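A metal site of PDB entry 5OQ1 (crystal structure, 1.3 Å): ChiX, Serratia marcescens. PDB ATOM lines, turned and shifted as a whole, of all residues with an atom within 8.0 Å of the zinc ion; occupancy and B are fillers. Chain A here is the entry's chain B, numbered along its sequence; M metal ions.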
ATOM      1  N   SER A  47      22.835 -24.612   7.551  1.00  0.00           N
ATOM      2  CA  SER A  47      23.195 -25.817   6.820  1.00  0.00           C
ATOM      3  C   SER A  47      23.870 -25.491   5.483  1.00  0.00           C
ATOM      4  O   SER A  47      24.656 -26.290   4.975  1.00  0.00           O
ATOM      5  CB  SER A  47      21.998 -26.735   6.586  1.00  0.00           C
ATOM      6  OG  SER A  47      21.107 -26.146   5.688  1.00  0.00           O
ATOM      7  N   GLU A  48      23.597 -24.309   4.923  1.00  0.00           N
ATOM      8  CA  GLU A  48      24.195 -23.905   3.660  1.00  0.00           C
ATOM      9  C   GLU A  48      24.231 -22.384   3.592  1.00  0.00           C
ATOM     10  O   GLU A  48      23.193 -21.741   3.778  1.00  0.00           O
ATOM     11  CB  GLU A  48      23.446 -24.467   2.450  1.00  0.00           C
ATOM     12  CG  GLU A  48      24.162 -24.213   1.120  1.00  0.00           C
ATOM     13  CD  GLU A  48      23.512 -24.845  -0.100  1.00  0.00           C
ATOM     14  OE1 GLU A  48      22.299 -25.202  -0.100  1.00  0.00           O
ATOM     15  OE2 GLU A  48      24.239 -25.047  -1.080  1.00  0.00           O
ATOM     16  N   GLY A  49      25.403 -21.850   3.332  1.00  0.00           N
ATOM     17  CA  GLY A  49      25.538 -20.411   3.074  1.00  0.00           C
ATOM     18  C   GLY A  49      25.895 -20.251   1.631  1.00  0.00           C
ATOM     19  O   GLY A  49      25.026 -20.314   0.753  1.00  0.00           O
ATOM     20  N   ARG A  51      27.015 -21.439  -1.931  1.00  0.00           N
ATOM     21  CA  ARG A  51      26.774 -22.621  -2.755  1.00  0.00           C
ATOM     22  C   ARG A  51      27.673 -22.531  -3.972  1.00  0.00           C
ATOM     23  O   ARG A  51      27.889 -21.445  -4.491  1.00  0.00           O
ATOM     24  CB  ARG A  51      25.320 -22.616  -3.189  1.00  0.00           C
ATOM     25  CG  ARG A  51      24.902 -23.804  -4.041  1.00  0.00           C
ATOM     26  CD  ARG A  51      23.457 -23.671  -4.386  1.00  0.00           C
ATOM     27  NE  ARG A  51      22.609 -23.867  -3.223  1.00  0.00           N
ATOM     28  CZ  ARG A  51      21.342 -23.480  -3.135  1.00  0.00           C
ATOM     29  NH1 ARG A  51      20.733 -22.863  -4.113  1.00  0.00           N
ATOM     30  NH2 ARG A  51      20.646 -23.722  -2.039  1.00  0.00           N
ATOM     31  N   ARG A  55      26.955 -27.186  -7.783  1.00  0.00           N
ATOM     32  CA  ARG A  55      25.739 -27.562  -7.081  1.00  0.00           C
ATOM     33  C   ARG A  55      24.517 -26.860  -7.642  1.00  0.00           C
ATOM     34  O   ARG A  55      23.468 -27.475  -7.814  1.00  0.00           O
ATOM     35  CB  ARG A  55      25.907 -27.246  -5.612  1.00  0.00           C
ATOM     36  CG  ARG A  55      24.701 -27.561  -4.784  1.00  0.00           C
ATOM     37  CD  ARG A  55      25.088 -27.761  -3.348  1.00  0.00           C
ATOM     38  NE  ARG A  55      23.980 -27.488  -2.459  1.00  0.00           N
ATOM     39  CZ  ARG A  55      22.917 -28.246  -2.287  1.00  0.00           C
ATOM     40  NH1 ARG A  55      21.973 -27.860  -1.417  1.00  0.00           N
ATOM     41  NH2 ARG A  55      22.740 -29.374  -2.996  1.00  0.00           N
ATOM     42  N   GLN A  56      24.655 -25.573  -7.949  1.00  0.00           N
ATOM     43  CA  GLN A  56      23.511 -24.873  -8.521  1.00  0.00           C
ATOM     44  C   GLN A  56      23.116 -25.451  -9.897  1.00  0.00           C
ATOM     45  O   GLN A  56      21.921 -25.620 -10.208  1.00  0.00           O
ATOM     46  CB  GLN A  56      23.763 -23.372  -8.615  1.00  0.00           C
ATOM     47  CG  GLN A  56      22.537 -22.542  -8.987  1.00  0.00           C
ATOM     48  CD  GLN A  56      21.499 -22.492  -7.872  1.00  0.00           C
ATOM     49  OE1 GLN A  56      21.846 -22.595  -6.703  1.00  0.00           O
ATOM     50  NE2 GLN A  56      20.253 -22.266  -8.225  1.00  0.00           N
ATOM     51  N   MET A  59      21.172 -28.513  -9.346  1.00  0.00           N
ATOM     52  CA  MET A  59      19.822 -28.205  -8.942  1.00  0.00           C
ATOM     53  C   MET A  59      18.952 -27.858 -10.167  1.00  0.00           C
ATOM     54  O   MET A  59      17.815 -28.252 -10.245  1.00  0.00           O
ATOM     55  CB  MET A  59      19.812 -27.100  -7.894  1.00  0.00           C
ATOM     56  CG  MET A  59      20.376 -27.544  -6.564  1.00  0.00           C
ATOM     57  SD  MET A  59      20.611 -26.151  -5.437  1.00  0.00           S
ATOM     58  CE  MET A  59      18.928 -25.622  -5.248  1.00  0.00           C
ATOM     59  N   SER A  70      21.258 -17.550  -8.172  1.00  0.00           N
ATOM     60  CA  SER A  70      20.872 -17.835  -6.809  1.00  0.00           C
ATOM     61  C   SER A  70      21.539 -16.856  -5.858  1.00  0.00           C
ATOM     62  O   SER A  70      22.742 -16.623  -5.975  1.00  0.00           O
ATOM     63  CB  SER A  70      21.288 -19.257  -6.382  1.00  0.00           C
ATOM     64  OG  SER A  70      21.147 -19.453  -4.979  1.00  0.00           O
ATOM     65  N   ARG A  71      20.784 -16.345  -4.907  1.00  0.00           N
ATOM     66  CA  ARG A  71      21.362 -15.564  -3.870  1.00  0.00           C
ATOM     67  C   ARG A  71      22.446 -16.325  -3.087  1.00  0.00           C
ATOM     68  O   ARG A  71      23.328 -15.709  -2.497  1.00  0.00           O
ATOM     69  CB  ARG A  71      20.273 -15.014  -2.930  1.00  0.00           C
ATOM     70  CG  ARG A  71      19.246 -14.091  -3.565  1.00  0.00           C
ATOM     71  CD  ARG A  71      19.373 -12.675  -3.128  1.00  0.00           C
ATOM     72  NE  ARG A  71      20.506 -12.049  -3.748  1.00  0.00           N
ATOM     73  CZ  ARG A  71      20.810 -10.761  -3.614  1.00  0.00           C
ATOM     74  NH1 ARG A  71      20.157 -10.011  -2.732  1.00  0.00           N
ATOM     75  NH2 ARG A  71      21.831 -10.261  -4.325  1.00  0.00           N
ATOM     76  N   HIS A  72      22.362 -17.657  -3.043  1.00  0.00           N
ATOM     77  CA  HIS A  72      23.418 -18.429  -2.374  1.00  0.00           C
ATOM     78  C   HIS A  72      24.789 -18.344  -3.030  1.00  0.00           C
ATOM     79  O   HIS A  72      25.784 -18.474  -2.366  1.00  0.00           O
ATOM     80  CB  HIS A  72      23.068 -19.925  -2.261  1.00  0.00           C
ATOM     81  CG  HIS A  72      21.998 -20.271  -1.251  1.00  0.00           C
ATOM     82  ND1 HIS A  72      22.264 -20.405   0.090  1.00  0.00           N
ATOM     83  CD2 HIS A  72      20.661 -20.414  -1.390  1.00  0.00           C
ATOM     84  CE1 HIS A  72      21.150 -20.728   0.728  1.00  0.00           C
ATOM     85  NE2 HIS A  72      20.158 -20.724  -0.152  1.00  0.00           N
ATOM     86  N   ALA A  77      22.407 -15.420   0.872  1.00  0.00           N
ATOM     87  CA  ALA A  77      21.391 -16.326   1.427  1.00  0.00           C
ATOM     88  C   ALA A  77      21.989 -17.368   2.326  1.00  0.00           C
ATOM     89  O   ALA A  77      23.158 -17.753   2.164  1.00  0.00           O
ATOM     90  CB  ALA A  77      20.602 -16.976   0.303  1.00  0.00           C
ATOM     91  N   VAL A  78      21.155 -17.816   3.268  1.00  0.00           N
ATOM     92  CA  VAL A  78      21.474 -18.972   4.056  1.00  0.00           C
ATOM     93  C   VAL A  78      20.243 -19.873   4.110  1.00  0.00           C
ATOM     94  O   VAL A  78      19.104 -19.420   4.070  1.00  0.00           O
ATOM     95  CB  VAL A  78      21.872 -18.612   5.513  1.00  0.00           C
ATOM     96  CG1 VAL A  78      23.152 -17.813   5.484  1.00  0.00           C
ATOM     97  CG2 VAL A  78      20.771 -17.839   6.238  1.00  0.00           C
ATOM     98  N   ASP A  79      20.498 -21.175   4.298  1.00  0.00           N
ATOM     99  CA  ASP A  79      19.486 -22.130   4.700  1.00  0.00           C
ATOM    100  C   ASP A  79      19.845 -22.562   6.096  1.00  0.00           C
ATOM    101  O   ASP A  79      20.959 -22.951   6.355  1.00  0.00           O
ATOM    102  CB  ASP A  79      19.414 -23.342   3.774  1.00  0.00           C
ATOM    103  CG  ASP A  79      18.935 -23.021   2.359  1.00  0.00           C
ATOM    104  OD1 ASP A  79      18.416 -21.902   2.116  1.00  0.00           O
ATOM    105  OD2 ASP A  79      18.957 -23.926   1.505  1.00  0.00           O
ATOM    106  N   VAL A  80      18.856 -22.507   6.967  1.00  0.00           N
ATOM    107  CA  VAL A  80      19.036 -22.927   8.337  1.00  0.00           C
ATOM    108  C   VAL A  80      18.430 -24.306   8.570  1.00  0.00           C
ATOM    109  O   VAL A  80      17.571 -24.746   7.809  1.00  0.00           O
ATOM    110  CB  VAL A  80      18.407 -21.948   9.358  1.00  0.00           C
ATOM    111  CG1 VAL A  80      18.952 -20.562   9.164  1.00  0.00           C
ATOM    112  CG2 VAL A  80      16.874 -21.912   9.264  1.00  0.00           C
ATOM    113  N   GLY A 116      11.852 -17.819   3.080  1.00  0.00           N
ATOM    114  CA  GLY A 116      11.173 -18.747   2.191  1.00  0.00           C
ATOM    115  C   GLY A 116       9.855 -19.257   2.708  1.00  0.00           C
ATOM    116  O   GLY A 116       9.061 -19.724   1.934  1.00  0.00           O
ATOM    117  N   TRP A 119       7.440 -17.267   0.768  1.00  0.00           N
ATOM    118  CA  TRP A 119       7.418 -17.316  -0.692  1.00  0.00           C
ATOM    119  C   TRP A 119       5.967 -17.357  -1.066  1.00  0.00           C
ATOM    120  O   TRP A 119       5.125 -17.869  -0.328  1.00  0.00           O
ATOM    121  CB  TRP A 119       8.139 -18.536  -1.269  1.00  0.00           C
ATOM    122  CG  TRP A 119       9.643 -18.473  -1.208  1.00  0.00           C
ATOM    123  CD1 TRP A 119      10.421 -17.339  -1.235  1.00  0.00           C
ATOM    124  CD2 TRP A 119      10.552 -19.575  -1.186  1.00  0.00           C
ATOM    125  NE1 TRP A 119      11.738 -17.672  -1.215  1.00  0.00           N
ATOM    126  CE2 TRP A 119      11.840 -19.041  -1.167  1.00  0.00           C
ATOM    127  CE3 TRP A 119      10.397 -20.973  -1.138  1.00  0.00           C
ATOM    128  CZ2 TRP A 119      12.958 -19.849  -1.108  1.00  0.00           C
ATOM    129  CZ3 TRP A 119      11.538 -21.761  -1.077  1.00  0.00           C
ATOM    130  CH2 TRP A 119      12.781 -21.188  -1.039  1.00  0.00           C
ATOM    131  N   ASP A 124       8.913 -22.798   2.065  1.00  0.00           N
ATOM    132  CA  ASP A 124       9.867 -23.703   2.670  1.00  0.00           C
ATOM    133  C   ASP A 124      10.662 -22.946   3.724  1.00  0.00           C
ATOM    134  O   ASP A 124      11.183 -21.866   3.461  1.00  0.00           O
ATOM    135  CB  ASP A 124      10.794 -24.343   1.622  1.00  0.00           C
ATOM    136  CG  ASP A 124      11.510 -25.588   2.144  1.00  0.00           C
ATOM    137  OD1 ASP A 124      10.858 -26.398   2.862  1.00  0.00           O
ATOM    138  OD2 ASP A 124      12.707 -25.793   1.833  1.00  0.00           O
ATOM    139  N   PRO A 126      13.598 -23.289   5.514  1.00  0.00           N
ATOM    140  CA  PRO A 126      15.004 -22.958   5.787  1.00  0.00           C
ATOM    141  C   PRO A 126      15.595 -21.681   5.233  1.00  0.00           C
ATOM    142  O   PRO A 126      16.598 -21.234   5.783  1.00  0.00           O
ATOM    143  CB  PRO A 126      15.738 -24.126   5.164  1.00  0.00           C
ATOM    144  CG  PRO A 126      14.784 -25.279   5.375  1.00  0.00           C
ATOM    145  CD  PRO A 126      13.443 -24.687   5.051  1.00  0.00           C
ATOM    146  N   HIS A 127      15.044 -21.170   4.143  1.00  0.00           N
ATOM    147  CA  HIS A 127      15.767 -20.176   3.346  1.00  0.00           C
ATOM    148  C   HIS A 127      15.518 -18.726   3.838  1.00  0.00           C
ATOM    149  O   HIS A 127      14.381 -18.303   4.009  1.00  0.00           O
ATOM    150  CB  HIS A 127      15.321 -20.291   1.892  1.00  0.00           C
ATOM    151  CG  HIS A 127      15.969 -19.329   0.967  1.00  0.00           C
ATOM    152  ND1 HIS A 127      17.131 -19.622   0.295  1.00  0.00           N
ATOM    153  CD2 HIS A 127      15.617 -18.092   0.592  1.00  0.00           C
ATOM    154  CE1 HIS A 127      17.469 -18.588  -0.447  1.00  0.00           C
ATOM    155  NE2 HIS A 127      16.549 -17.661  -0.292  1.00  0.00           N
ATOM    156  N   PHE A 128      16.619 -17.994   4.003  1.00  0.00           N
ATOM    157  CA  PHE A 128      16.599 -16.553   4.292  1.00  0.00           C
ATOM    158  C   PHE A 128      17.551 -15.847   3.353  1.00  0.00           C
ATOM    159  O   PHE A 128      18.613 -16.406   3.053  1.00  0.00           O
ATOM    160  CB  PHE A 128      17.000 -16.265   5.721  1.00  0.00           C
ATOM    161  CG  PHE A 128      16.076 -16.806   6.737  1.00  0.00           C
ATOM    162  CD1 PHE A 128      16.216 -18.096   7.230  1.00  0.00           C
ATOM    163  CD2 PHE A 128      15.032 -16.031   7.190  1.00  0.00           C
ATOM    164  CE1 PHE A 128      15.346 -18.589   8.183  1.00  0.00           C
ATOM    165  CE2 PHE A 128      14.174 -16.523   8.136  1.00  0.00           C
ATOM    166  CZ  PHE A 128      14.333 -17.799   8.637  1.00  0.00           C
ATOM    167  N   GLN A 129      17.199 -14.675   2.866  1.00  0.00           N
ATOM    168  CA  GLN A 129      18.086 -13.913   1.999  1.00  0.00           C
ATOM    169  C   GLN A 129      17.936 -12.417   2.163  1.00  0.00           C
ATOM    170  O   GLN A 129      16.884 -11.916   2.544  1.00  0.00           O
ATOM    171  CB  GLN A 129      17.851 -14.250   0.552  1.00  0.00           C
ATOM    172  CG  GLN A 129      16.472 -13.860   0.020  1.00  0.00           C
ATOM    173  CD  GLN A 129      16.258 -14.266  -1.413  1.00  0.00           C
ATOM    174  OE1 GLN A 129      16.549 -15.406  -1.794  1.00  0.00           O
ATOM    175  NE2 GLN A 129      15.735 -13.352  -2.227  1.00  0.00           N
HETATM  176 ZN    ZN M   1      18.270 -21.381   0.263  1.00  0.00          ZN
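The side-chain carboxylate of Asp 79 lies within salt-bridge range of the guanidinium group of Arg 51, 3.9 Å away. O of Glu 48 lies within hydrogen-bond range of N of Asp 79 (2.8 Å). O of Asp 79 is in hydrogen-bond range of N of Ser 47 (2.8 Å). N of Arg 51 lies within hydrogen-bond range of O of His 72 (3.2 Å). A ring nitrogen (ND1) of His 72 lies within hydrogen-bond range of the backbone carbonyl oxygen (O) of Ala 77, at 3.5 Å. The backbone NH (N) of His 72 sits at hydrogen-bond distance from the side-chain hydroxyl (OG) of Ser 70, at 2.9 Å. ND1 of His 72 lies within hydrogen-bond range of O of Gly 49. OE1 of Gln 129 lies within hydrogen-bond range of NE2 of His 127 (2.7 Å).
The zinc ion is bound by the side-chain carboxylate of Asp 79, a ring nitrogen (NE2) of His 72 and a ring nitrogen (ND1) of His 127.
The nearest printed residue that does not touch the zinc ion is Arg 51 (4.1 Å).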
